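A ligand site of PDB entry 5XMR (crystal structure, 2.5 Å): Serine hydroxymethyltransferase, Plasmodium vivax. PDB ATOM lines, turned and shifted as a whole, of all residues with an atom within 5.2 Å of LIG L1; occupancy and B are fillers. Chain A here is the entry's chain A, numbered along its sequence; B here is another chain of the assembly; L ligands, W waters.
OG of Ser 34 is in hydrogen-bond range of O6 of LIG L1, at 2.5 Å. A ring nitrogen (NE2) of His 211 sits at hydrogen-bond distance from an oxygen (O7) of LIG L1, 2.6 Å away. An oxygen (O4) of LIG L1 lies within hydrogen-bond range of the side-chain hydroxyl (OH) of Tyr 54 of chain B (2.7 Å). N of Ser 102 sits at hydrogen-bond distance from O3 of LIG L1 (3.0 Å). OG of Ser 102 is in hydrogen-bond range of O3 of LIG L1, 2.8 Å away. O5 of LIG L1 lies within hydrogen-bond range of OG of Ser 100 (2.9 Å). O6 of LIG L1 lies within hydrogen-bond range of OH of Tyr 64 of chain B, at 2.9 Å. NH2 of Arg 371 is in salt-bridge range of O6 of LIG L1, at 3.0 Å. O4 of LIG L1 sits at hydrogen-bond distance from N of Gly 272 of chain B (3.0 Å). O5 of LIG L1 sits close to NE2 of His 236, 3.2 Å away. N of Gly 101 lies within hydrogen-bond range of O5 of LIG L1 (3.3 Å). The side-chain hydroxyl of Thr 183 is in hydrogen-bond range of an oxygen (O3) of LG2 L2. The side-chain carboxylate (OE2) of Glu 56 of chain B lies within hydrogen-bond range of a nitrogen (N3) of LG2 L2 (2.9 Å).
The guanidinium group of Arg 371 sits close to a ring nitrogen (NE2) of His 211. The backbone carbonyl oxygen (O) of Thr 183 is in hydrogen-bond range of a ring nitrogen (NE2) of His 211, 3.1 Å away. OH of Tyr 54 of chain B sits at hydrogen-bond distance from NE2 of His 236, 3.2 Å away. OG of Ser 102 is in hydrogen-bond range of N of Gly 271 of chain B, at 3.3 Å. The side-chain hydroxyl of Tyr 64 of chain B is in hydrogen-bond range of the guanidinium group of Arg 371 (3.5 Å). The side-chain carboxylate of Asp 208 sits close to the backbone NH of Ser 210 (3.4 Å). The side-chain carboxylate (OD2) of Asp 208 sits at hydrogen-bond distance from the side-chain amide nitrogen (ND2) of Asn 105 (2.8 Å). OG1 of Thr 131 is in hydrogen-bond range of ND2 of Asn 105, 2.8 Å away.
The side-chain carboxylate (OD2) of Asp 208 lies close to a nitrogen (N1) of LIG L1. Residues that only touch LIG L1: Thr 183 (3.0 Å), His 129 (3.2 Å), Lys 237 (3.4 Å), Glu 56 of chain B (3.6 Å), Ser 210 (3.6 Å), Gly 271 of chain B (3.6 Å), Tyr 182 (3.7 Å), Asn 105 (3.9 Å) and Thr 234 (3.9 Å). Within 4 Å of LIG L1: Ser 34, Ser 100, Gly 101, Ser 102, Asn 105, His 129, Tyr 182, Thr 183, Asp 208, Ser 210, His 211, Thr 234, His 236, Lys 237, Arg 371, Tyr 54 of chain B, Glu 56 of chain B, Tyr 64 of chain B, Gly 271 of chain B and Gly 272 of chain B. The nearest printed residue that does not touch LIG L1 is His 132 (4.2 Å).
Water W3 lies within hydrogen-bond range of an oxygen (O3) of LIG L1 (2.7 Å), the backbone carbonyl oxygen of Gly 272 of chain B (3.0 Å), the backbone NH of Gly 271 of chain B (3.2 Å) and the side-chain hydroxyl of Ser 100 (3.2 Å). Water W2 lies within hydrogen-bond range of OE2 of Glu 56 of chain B (2.7 Å), O4 of LIG L1 (2.8 Å) and NE2 of His 129 (3.1 Å). Water W1 lies within hydrogen-bond range of NH2 of Arg 243 (2.6 Å), O5 of LIG L1 (2.9 Å), O of Gly 272 of chain B (3.2 Å), OG of Ser 100 (3.2 Å) and NE2 of His 236 (3.5 Å).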
ATOM      1  N   ILE A  32       1.601  -5.803  -5.751  1.00  0.00           N
ATOM      2  CA  ILE A  32       1.284  -4.450  -6.271  1.00  0.00           C
ATOM      3  C   ILE A  32       0.569  -3.682  -5.159  1.00  0.00           C
ATOM      4  O   ILE A  32      -0.487  -4.069  -4.730  1.00  0.00           O
ATOM      5  CB  ILE A  32       0.401  -4.464  -7.540  1.00  0.00           C
ATOM      6  CG1 ILE A  32       1.033  -5.299  -8.661  1.00  0.00           C
ATOM      7  CG2 ILE A  32       0.178  -3.046  -8.011  1.00  0.00           C
ATOM      8  CD1 ILE A  32       2.226  -4.665  -9.340  1.00  0.00           C
ATOM      9  N   SER A  34      -1.111  -1.048  -4.877  1.00  0.00           N
ATOM     10  CA  SER A  34      -2.436  -0.518  -5.204  1.00  0.00           C
ATOM     11  C   SER A  34      -3.511  -1.560  -5.518  1.00  0.00           C
ATOM     12  O   SER A  34      -4.658  -1.190  -5.748  1.00  0.00           O
ATOM     13  CB  SER A  34      -2.286   0.391  -6.404  1.00  0.00           C
ATOM     14  OG  SER A  34      -1.574  -0.275  -7.414  1.00  0.00           O
ATOM     15  N   SER A 100     -13.265   7.136 -11.260  1.00  0.00           N
ATOM     16  CA  SER A 100     -11.980   6.601 -10.856  1.00  0.00           C
ATOM     17  C   SER A 100     -11.166   7.700 -10.193  1.00  0.00           C
ATOM     18  O   SER A 100     -11.521   8.898 -10.280  1.00  0.00           O
ATOM     19  CB  SER A 100     -11.211   6.011 -12.075  1.00  0.00           C
ATOM     20  OG  SER A 100     -10.603   4.737 -11.805  1.00  0.00           O
ATOM     21  N   GLY A 101     -10.053   7.327  -9.574  1.00  0.00           N
ATOM     22  CA  GLY A 101      -9.281   8.305  -8.836  1.00  0.00           C
ATOM     23  C   GLY A 101      -8.792   9.521  -9.618  1.00  0.00           C
ATOM     24  O   GLY A 101      -8.719  10.609  -9.075  1.00  0.00           O
ATOM     25  N   SER A 102      -8.429   9.319 -10.872  1.00  0.00           N
ATOM     26  CA  SER A 102      -7.866  10.409 -11.683  1.00  0.00           C
ATOM     27  C   SER A 102      -8.965  11.373 -12.139  1.00  0.00           C
ATOM     28  O   SER A 102      -8.786  12.574 -12.165  1.00  0.00           O
ATOM     29  CB  SER A 102      -7.065   9.862 -12.880  1.00  0.00           C
ATOM     30  OG  SER A 102      -6.044   8.931 -12.460  1.00  0.00           O
ATOM     31  N   ALA A 103     -10.116  10.829 -12.483  1.00  0.00           N
ATOM     32  CA  ALA A 103     -11.287  11.648 -12.695  1.00  0.00           C
ATOM     33  C   ALA A 103     -11.614  12.518 -11.450  1.00  0.00           C
ATOM     34  O   ALA A 103     -11.734  13.740 -11.572  1.00  0.00           O
ATOM     35  CB  ALA A 103     -12.457  10.767 -13.064  1.00  0.00           C
ATOM     36  N   ASN A 105      -9.713  13.422  -8.787  1.00  0.00           N
ATOM     37  CA  ASN A 105      -8.728  14.486  -8.532  1.00  0.00           C
ATOM     38  C   ASN A 105      -8.828  15.699  -9.476  1.00  0.00           C
ATOM     39  O   ASN A 105      -8.717  16.822  -8.998  1.00  0.00           O
ATOM     40  CB  ASN A 105      -7.298  13.950  -8.557  1.00  0.00           C
ATOM     41  CG  ASN A 105      -6.983  13.040  -7.379  1.00  0.00           C
ATOM     42  OD1 ASN A 105      -7.750  12.920  -6.431  1.00  0.00           O
ATOM     43  ND2 ASN A 105      -5.824  12.394  -7.440  1.00  0.00           N
ATOM     44  N   HIS A 129       1.361  11.357  -7.537  1.00  0.00           N
ATOM     45  CA  HIS A 129       0.594  10.876  -8.656  1.00  0.00           C
ATOM     46  C   HIS A 129       0.669  11.818  -9.840  1.00  0.00           C
ATOM     47  O   HIS A 129       1.112  12.968  -9.713  1.00  0.00           O
ATOM     48  CB  HIS A 129      -0.876  10.661  -8.254  1.00  0.00           C
ATOM     49  CG  HIS A 129      -1.635   9.740  -9.158  1.00  0.00           C
ATOM     50  ND1 HIS A 129      -2.644  10.179  -9.989  1.00  0.00           N
ATOM     51  CD2 HIS A 129      -1.487   8.422  -9.416  1.00  0.00           C
ATOM     52  CE1 HIS A 129      -3.107   9.164 -10.690  1.00  0.00           C
ATOM     53  NE2 HIS A 129      -2.421   8.081 -10.356  1.00  0.00           N
ATOM     54  N   THR A 131      -1.948  12.969 -11.524  1.00  0.00           N
ATOM     55  CA  THR A 131      -2.993  13.977 -11.258  1.00  0.00           C
ATOM     56  C   THR A 131      -2.650  15.090 -10.260  1.00  0.00           C
ATOM     57  O   THR A 131      -3.484  15.961  -9.996  1.00  0.00           O
ATOM     58  CB  THR A 131      -4.294  13.335 -10.753  1.00  0.00           C
ATOM     59  OG1 THR A 131      -4.045  12.571  -9.569  1.00  0.00           O
ATOM     60  CG2 THR A 131      -4.876  12.440 -11.827  1.00  0.00           C
ATOM     61  N   HIS A 132      -1.428  15.084  -9.707  1.00  0.00           N
ATOM     62  CA  HIS A 132      -0.981  16.137  -8.778  1.00  0.00           C
ATOM     63  C   HIS A 132      -0.152  17.162  -9.517  1.00  0.00           C
ATOM     64  O   HIS A 132       0.697  17.840  -8.918  1.00  0.00           O
ATOM     65  CB  HIS A 132      -0.232  15.530  -7.574  1.00  0.00           C
ATOM     66  CG  HIS A 132      -1.016  14.479  -6.838  1.00  0.00           C
ATOM     67  ND1 HIS A 132      -0.460  13.666  -5.884  1.00  0.00           N
ATOM     68  CD2 HIS A 132      -2.308  14.089  -6.947  1.00  0.00           C
ATOM     69  CE1 HIS A 132      -1.374  12.838  -5.408  1.00  0.00           C
ATOM     70  NE2 HIS A 132      -2.507  13.079  -6.047  1.00  0.00           N
ATOM     71  N   GLY A 181      -0.600  13.445   0.154  1.00  0.00           N
ATOM     72  CA  GLY A 181      -1.155  12.096  -0.007  1.00  0.00           C
ATOM     73  C   GLY A 181      -0.683  11.637  -1.377  1.00  0.00           C
ATOM     74  O   GLY A 181      -0.764  12.388  -2.355  1.00  0.00           O
ATOM     75  N   TYR A 182      -0.137  10.425  -1.438  1.00  0.00           N
ATOM     76  CA  TYR A 182       0.757  10.073  -2.536  1.00  0.00           C
ATOM     77  C   TYR A 182       0.606   8.640  -3.014  1.00  0.00           C
ATOM     78  O   TYR A 182      -0.145   7.873  -2.429  1.00  0.00           O
ATOM     79  CB  TYR A 182       2.181  10.340  -2.079  1.00  0.00           C
ATOM     80  CG  TYR A 182       2.402  11.689  -1.422  1.00  0.00           C
ATOM     81  CD1 TYR A 182       2.292  12.866  -2.158  1.00  0.00           C
ATOM     82  CD2 TYR A 182       2.752  11.794  -0.084  1.00  0.00           C
ATOM     83  CE1 TYR A 182       2.540  14.094  -1.568  1.00  0.00           C
ATOM     84  CE2 TYR A 182       3.018  13.010   0.510  1.00  0.00           C
ATOM     85  CZ  TYR A 182       2.912  14.171  -0.238  1.00  0.00           C
ATOM     86  OH  TYR A 182       3.135  15.405   0.336  1.00  0.00           O
ATOM     87  N   THR A 183       1.298   8.299  -4.096  1.00  0.00           N
ATOM     88  CA  THR A 183       1.101   6.973  -4.725  1.00  0.00           C
ATOM     89  C   THR A 183       2.113   5.955  -4.232  1.00  0.00           C
ATOM     90  O   THR A 183       1.764   4.785  -4.006  1.00  0.00           O
ATOM     91  CB  THR A 183       1.005   6.978  -6.282  1.00  0.00           C
ATOM     92  OG1 THR A 183       2.110   6.264  -6.867  1.00  0.00           O
ATOM     93  CG2 THR A 183       0.933   8.324  -6.825  1.00  0.00           C
ATOM     94  N   ASP A 208      -4.958  13.358  -0.798  1.00  0.00           N
ATOM     95  CA  ASP A 208      -5.272  12.200  -1.614  1.00  0.00           C
ATOM     96  C   ASP A 208      -4.792  10.972  -0.869  1.00  0.00           C
ATOM     97  O   ASP A 208      -3.598  10.631  -0.923  1.00  0.00           O
ATOM     98  CB  ASP A 208      -4.557  12.315  -2.953  1.00  0.00           C
ATOM     99  CG  ASP A 208      -4.963  11.239  -3.936  1.00  0.00           C
ATOM    100  OD1 ASP A 208      -5.558  10.227  -3.532  1.00  0.00           O
ATOM    101  OD2 ASP A 208      -4.677  11.425  -5.131  1.00  0.00           O
ATOM    102  N   SER A 210      -5.830   7.734  -1.207  1.00  0.00           N
ATOM    103  CA  SER A 210      -6.168   6.515  -1.953  1.00  0.00           C
ATOM    104  C   SER A 210      -5.354   5.313  -1.524  1.00  0.00           C
ATOM    105  O   SER A 210      -5.887   4.209  -1.345  1.00  0.00           O
ATOM    106  CB  SER A 210      -5.924   6.751  -3.440  1.00  0.00           C
ATOM    107  OG  SER A 210      -6.406   8.034  -3.843  1.00  0.00           O
ATOM    108  N   HIS A 211      -4.042   5.523  -1.346  1.00  0.00           N
ATOM    109  CA  HIS A 211      -3.178   4.432  -0.876  1.00  0.00           C
ATOM    110  C   HIS A 211      -3.385   4.042   0.587  1.00  0.00           C
ATOM    111  O   HIS A 211      -3.269   2.869   0.941  1.00  0.00           O
ATOM    112  CB  HIS A 211      -1.699   4.674  -1.226  1.00  0.00           C
ATOM    113  CG  HIS A 211      -1.317   4.010  -2.515  1.00  0.00           C
ATOM    114  ND1 HIS A 211      -0.885   2.708  -2.567  1.00  0.00           N
ATOM    115  CD2 HIS A 211      -1.406   4.424  -3.796  1.00  0.00           C
ATOM    116  CE1 HIS A 211      -0.692   2.358  -3.822  1.00  0.00           C
ATOM    117  NE2 HIS A 211      -0.989   3.390  -4.587  1.00  0.00           N
ATOM    118  N   THR A 234      -9.561   6.777  -3.846  1.00  0.00           N
ATOM    119  CA  THR A 234     -10.111   5.674  -4.597  1.00  0.00           C
ATOM    120  C   THR A 234     -10.676   4.663  -3.622  1.00  0.00           C
ATOM    121  O   THR A 234     -10.351   4.680  -2.429  1.00  0.00           O
ATOM    122  CB  THR A 234      -9.068   4.979  -5.491  1.00  0.00           C
ATOM    123  OG1 THR A 234      -7.947   4.579  -4.688  1.00  0.00           O
ATOM    124  CG2 THR A 234      -8.633   5.936  -6.605  1.00  0.00           C
ATOM    125  N   HIS A 236     -10.596   1.166  -4.524  1.00  0.00           N
ATOM    126  CA  HIS A 236     -10.186  -0.176  -5.044  1.00  0.00           C
ATOM    127  C   HIS A 236      -8.830  -0.685  -4.549  1.00  0.00           C
ATOM    128  O   HIS A 236      -8.457  -1.825  -4.843  1.00  0.00           O
ATOM    129  CB  HIS A 236     -10.223  -0.265  -6.576  1.00  0.00           C
ATOM    130  CG  HIS A 236      -9.573   0.869  -7.281  1.00  0.00           C
ATOM    131  ND1 HIS A 236     -10.210   2.077  -7.510  1.00  0.00           N
ATOM    132  CD2 HIS A 236      -8.372   0.969  -7.892  1.00  0.00           C
ATOM    133  CE1 HIS A 236      -9.416   2.878  -8.207  1.00  0.00           C
ATOM    134  NE2 HIS A 236      -8.290   2.221  -8.445  1.00  0.00           N
ATOM    135  N   LYS A 237      -8.121   0.133  -3.796  1.00  0.00           N
ATOM    136  CA  LYS A 237      -6.847  -0.249  -3.277  1.00  0.00           C
ATOM    137  C   LYS A 237      -7.052  -0.878  -1.906  1.00  0.00           C
ATOM    138  O   LYS A 237      -7.766  -1.880  -1.785  1.00  0.00           O
ATOM    139  CB  LYS A 237      -5.923   0.934  -3.259  1.00  0.00           C
ATOM    140  CG  LYS A 237      -5.817   1.680  -4.565  1.00  0.00           C
ATOM    141  CD  LYS A 237      -4.857   2.816  -4.377  1.00  0.00           C
ATOM    142  CE  LYS A 237      -4.504   3.432  -5.681  1.00  0.00           C
ATOM    143  NZ  LYS A 237      -5.697   3.963  -6.362  1.00  0.00           N
ATOM    144  N   ARG A 243     -13.723  -0.333  -8.448  1.00  0.00           N
ATOM    145  CA  ARG A 243     -12.955   0.742  -9.056  1.00  0.00           C
ATOM    146  C   ARG A 243     -13.796   2.033  -9.129  1.00  0.00           C
ATOM    147  O   ARG A 243     -14.607   2.222 -10.039  1.00  0.00           O
ATOM    148  CB  ARG A 243     -12.408   0.374 -10.450  1.00  0.00           C
ATOM    149  CG  ARG A 243     -11.453  -0.813 -10.421  1.00  0.00           C
ATOM    150  CD  ARG A 243     -10.740  -1.010 -11.761  1.00  0.00           C
ATOM    151  NE  ARG A 243      -9.496  -0.258 -11.781  1.00  0.00           N
ATOM    152  CZ  ARG A 243      -8.355  -0.660 -11.216  1.00  0.00           C
ATOM    153  NH1 ARG A 243      -8.228  -1.838 -10.619  1.00  0.00           N
ATOM    154  NH2 ARG A 243      -7.314   0.147 -11.276  1.00  0.00           N
ATOM    155  N   ARG A 371       8.455  -1.215  -5.948  1.00  0.00           N
ATOM    156  CA  ARG A 371       7.495  -0.926  -4.923  1.00  0.00           C
ATOM    157  C   ARG A 371       6.665  -2.164  -4.658  1.00  0.00           C
ATOM    158  O   ARG A 371       6.195  -2.819  -5.587  1.00  0.00           O
ATOM    159  CB  ARG A 371       6.608   0.220  -5.373  1.00  0.00           C
ATOM    160  CG  ARG A 371       5.605   0.678  -4.331  1.00  0.00           C
ATOM    161  CD  ARG A 371       4.605   1.636  -4.959  1.00  0.00           C
ATOM    162  NE  ARG A 371       3.749   1.001  -5.944  1.00  0.00           N
ATOM    163  CZ  ARG A 371       2.558   1.419  -6.333  1.00  0.00           C
ATOM    164  NH1 ARG A 371       1.980   2.488  -5.788  1.00  0.00           N
ATOM    165  NH2 ARG A 371       1.908   0.750  -7.271  1.00  0.00           N
ATOM    166  N   TYR B  54      -4.402  -3.747 -12.152  1.00  0.00           N
ATOM    167  CA  TYR B  54      -3.925  -2.438 -12.561  1.00  0.00           C
ATOM    168  C   TYR B  54      -3.076  -2.610 -13.820  1.00  0.00           C
ATOM    169  O   TYR B  54      -2.039  -3.257 -13.788  1.00  0.00           O
ATOM    170  CB  TYR B  54      -3.073  -1.774 -11.447  1.00  0.00           C
ATOM    171  CG  TYR B  54      -3.687  -0.471 -10.964  1.00  0.00           C
ATOM    172  CD1 TYR B  54      -3.823   0.625 -11.822  1.00  0.00           C
ATOM    173  CD2 TYR B  54      -4.194  -0.352  -9.671  1.00  0.00           C
ATOM    174  CE1 TYR B  54      -4.428   1.789 -11.407  1.00  0.00           C
ATOM    175  CE2 TYR B  54      -4.795   0.826  -9.255  1.00  0.00           C
ATOM    176  CZ  TYR B  54      -4.910   1.873 -10.127  1.00  0.00           C
ATOM    177  OH  TYR B  54      -5.516   3.016  -9.717  1.00  0.00           O
ATOM    178  N   GLU B  56      -2.190   0.160 -16.238  1.00  0.00           N
ATOM    179  CA  GLU B  56      -1.962   1.458 -16.849  1.00  0.00           C
ATOM    180  C   GLU B  56      -1.072   1.326 -18.063  1.00  0.00           C
ATOM    181  O   GLU B  56      -0.085   0.597 -18.059  1.00  0.00           O
ATOM    182  CB  GLU B  56      -1.275   2.387 -15.848  1.00  0.00           C
ATOM    183  CG  GLU B  56      -2.175   2.834 -14.707  1.00  0.00           C
ATOM    184  CD  GLU B  56      -1.419   3.660 -13.683  1.00  0.00           C
ATOM    185  OE1 GLU B  56      -0.767   3.058 -12.816  1.00  0.00           O
ATOM    186  OE2 GLU B  56      -1.472   4.909 -13.767  1.00  0.00           O
ATOM    187  N   TYR B  64       3.231  -2.128 -15.909  1.00  0.00           N
ATOM    188  CA  TYR B  64       3.493  -3.334 -15.100  1.00  0.00           C
ATOM    189  C   TYR B  64       3.326  -4.593 -15.937  1.00  0.00           C
ATOM    190  O   TYR B  64       2.604  -4.591 -16.925  1.00  0.00           O
ATOM    191  CB  TYR B  64       2.550  -3.473 -13.907  1.00  0.00           C
ATOM    192  CG  TYR B  64       2.275  -2.248 -13.095  1.00  0.00           C
ATOM    193  CD1 TYR B  64       3.078  -1.115 -13.154  1.00  0.00           C
ATOM    194  CD2 TYR B  64       1.204  -2.244 -12.193  1.00  0.00           C
ATOM    195  CE1 TYR B  64       2.799  -0.026 -12.386  1.00  0.00           C
ATOM    196  CE2 TYR B  64       0.917  -1.153 -11.396  1.00  0.00           C
ATOM    197  CZ  TYR B  64       1.707  -0.031 -11.495  1.00  0.00           C
ATOM    198  OH  TYR B  64       1.380   1.047 -10.696  1.00  0.00           O
ATOM    199  N   GLN B 270      -6.931   9.859 -17.680  1.00  0.00           N
ATOM    200  CA  GLN B 270      -7.217   8.710 -16.831  1.00  0.00           C
ATOM    201  C   GLN B 270      -5.964   8.108 -16.288  1.00  0.00           C
ATOM    202  O   GLN B 270      -4.859   8.482 -16.686  1.00  0.00           O
ATOM    203  CB  GLN B 270      -8.006   7.642 -17.576  1.00  0.00           C
ATOM    204  CG  GLN B 270      -9.261   8.166 -18.219  1.00  0.00           C
ATOM    205  CD  GLN B 270     -10.229   7.093 -18.671  1.00  0.00           C
ATOM    206  OE1 GLN B 270     -11.413   7.391 -18.873  1.00  0.00           O
ATOM    207  NE2 GLN B 270      -9.758   5.864 -18.868  1.00  0.00           N
ATOM    208  N   GLY B 271      -6.152   7.218 -15.323  1.00  0.00           N
ATOM    209  CA  GLY B 271      -5.137   6.316 -14.827  1.00  0.00           C
ATOM    210  C   GLY B 271      -5.509   4.928 -15.304  1.00  0.00           C
ATOM    211  O   GLY B 271      -5.701   4.711 -16.497  1.00  0.00           O
ATOM    212  N   GLY B 272      -5.663   3.994 -14.371  1.00  0.00           N
ATOM    213  CA  GLY B 272      -5.797   2.590 -14.733  1.00  0.00           C
ATOM    214  C   GLY B 272      -7.088   2.289 -15.463  1.00  0.00           C
ATOM    215  O   GLY B 272      -8.132   2.838 -15.110  1.00  0.00           O
HETATM  216  N1  LIG L   1      -4.410   8.866  -6.696  1.00  0.00           N
HETATM  217  C1  LIG L   1      -3.350   8.243  -6.126  1.00  0.00           C
HETATM  218  C2  LIG L   1      -2.624   8.842  -4.956  1.00  0.00           C
HETATM  219  C3  LIG L   1      -2.903   6.952  -6.647  1.00  0.00           C
HETATM  220  O1  LIG L   1      -1.877   6.258  -6.147  1.00  0.00           O
HETATM  221  C4  LIG L   1      -3.588   6.365  -7.784  1.00  0.00           C
HETATM  222  C5  LIG L   1      -3.101   5.012  -8.314  1.00  0.00           C
HETATM  223  C6  LIG L   1      -4.735   7.160  -8.322  1.00  0.00           C
HETATM  224  C7  LIG L   1      -5.100   8.381  -7.766  1.00  0.00           C
HETATM  225  C8  LIG L   1      -5.404   6.497  -9.473  1.00  0.00           C
HETATM  226  O2  LIG L   1      -6.684   6.785  -9.924  1.00  0.00           O
HETATM  227  P1  LIG L   1      -7.164   5.720 -11.030  1.00  0.00           P
HETATM  228  O3  LIG L   1      -7.680   6.705 -12.057  1.00  0.00           O
HETATM  229  O4  LIG L   1      -5.952   4.958 -11.535  1.00  0.00           O
HETATM  230  O5  LIG L   1      -8.139   4.802 -10.345  1.00  0.00           O
HETATM  231  C9  LIG L   1      -0.812   2.825  -8.298  1.00  0.00           C
HETATM  232  O6  LIG L   1      -0.581   1.648  -8.591  1.00  0.00           O
HETATM  233  O7  LIG L   1      -0.659   3.218  -7.128  1.00  0.00           O
HETATM  234  C10 LIG L   1      -1.245   3.777  -9.370  1.00  0.00           C
HETATM  235  N2  LIG L   1      -1.751   5.003  -8.802  1.00  0.00           N
HETATM  236  C1  LG2 L   2       4.061   7.118  -9.417  1.00  0.00           C
HETATM  237  C2  LG2 L   2       4.866   6.281 -10.112  1.00  0.00           C
HETATM  238  C3  LG2 L   2       4.350   5.385 -11.229  1.00  0.00           C
HETATM  239  C4  LG2 L   2       2.937   5.754 -11.614  1.00  0.00           C
HETATM  240  C5  LG2 L   2       2.110   6.697 -10.846  1.00  0.00           C
HETATM  241  C6  LG2 L   2       6.122   6.175  -9.817  1.00  0.00           C
HETATM  242  C7  LG2 L   2       2.004   5.386 -12.734  1.00  0.00           C
HETATM  243  C8  LG2 L   2       2.198   4.475 -13.921  1.00  0.00           C
HETATM  244  C9  LG2 L   2       4.334   3.935 -10.685  1.00  0.00           C
HETATM  245  C10 LG2 L   2       4.229   2.898 -11.797  1.00  0.00           C
HETATM  246  C11 LG2 L   2       5.294   5.567 -12.427  1.00  0.00           C
HETATM  247  C12 LG2 L   2       6.537   4.894 -12.440  1.00  0.00           C
HETATM  248  C13 LG2 L   2       7.416   5.018 -13.504  1.00  0.00           C
HETATM  249  C14 LG2 L   2       7.095   5.841 -14.573  1.00  0.00           C
HETATM  250  C15 LG2 L   2       5.886   6.521 -14.590  1.00  0.00           C
HETATM  251  C16 LG2 L   2       4.985   6.395 -13.532  1.00  0.00           C
HETATM  252  O1  LG2 L   2       5.580  10.991 -19.385  1.00  0.00           O
HETATM  253  S1  LG2 L   2       4.786   9.799 -19.362  1.00  0.00           S
HETATM  254  O2  LG2 L   2       3.417  10.175 -19.362  1.00  0.00           O
HETATM  255  C17 LG2 L   2       4.881   8.913 -20.781  1.00  0.00           C
HETATM  256  C18 LG2 L   2       6.211   8.252 -21.093  1.00  0.00           C
HETATM  257  C19 LG2 L   2       7.453   8.796 -20.719  1.00  0.00           C
HETATM  258  C20 LG2 L   2       8.644   8.131 -21.041  1.00  0.00           C
HETATM  259  C21 LG2 L   2       8.601   6.922 -21.733  1.00  0.00           C
HETATM  260  C22 LG2 L   2       7.369   6.368 -22.108  1.00  0.00           C
HETATM  261  C23 LG2 L   2       6.184   7.039 -21.791  1.00  0.00           C
HETATM  262  C24 LG2 L   2       5.073   8.922 -18.056  1.00  0.00           C
HETATM  263  C25 LG2 L   2       4.072   8.128 -17.488  1.00  0.00           C
HETATM  264  C26 LG2 L   2       4.332   7.341 -16.369  1.00  0.00           C
HETATM  265  C27 LG2 L   2       6.341   8.941 -17.470  1.00  0.00           C
HETATM  266  C28 LG2 L   2       6.589   8.171 -16.343  1.00  0.00           C
HETATM  267  C29 LG2 L   2       5.589   7.369 -15.782  1.00  0.00           C
HETATM  268  C30 LG2 L   2       8.726   4.299 -13.486  1.00  0.00           C
HETATM  269  F1  LG2 L   2       8.789   3.300 -12.611  1.00  0.00           F
HETATM  270  F2  LG2 L   2       9.589   5.216 -13.119  1.00  0.00           F
HETATM  271  F3  LG2 L   2       9.011   3.868 -14.707  1.00  0.00           F
HETATM  272  C31 LG2 L   2       3.305   3.651  -9.583  1.00  0.00           C
HETATM  273  N1  LG2 L   2       7.254   6.106  -9.561  1.00  0.00           N
HETATM  274  N2  LG2 L   2       4.503   7.902  -8.414  1.00  0.00           N
HETATM  275  N3  LG2 L   2       0.863   6.069 -12.500  1.00  0.00           N
HETATM  276  N4  LG2 L   2       0.869   6.897 -11.354  1.00  0.00           N
HETATM  277  O3  LG2 L   2       2.629   7.244  -9.714  1.00  0.00           O
HETATM  278  O   HOH W   1      -8.418   2.358 -11.927  1.00  0.00           O
HETATM  279  O   HOH W   2      -3.210   5.502 -11.841  1.00  0.00           O
HETATM  280  O   HOH W   3      -8.723   5.614 -14.276  1.00  0.00           O
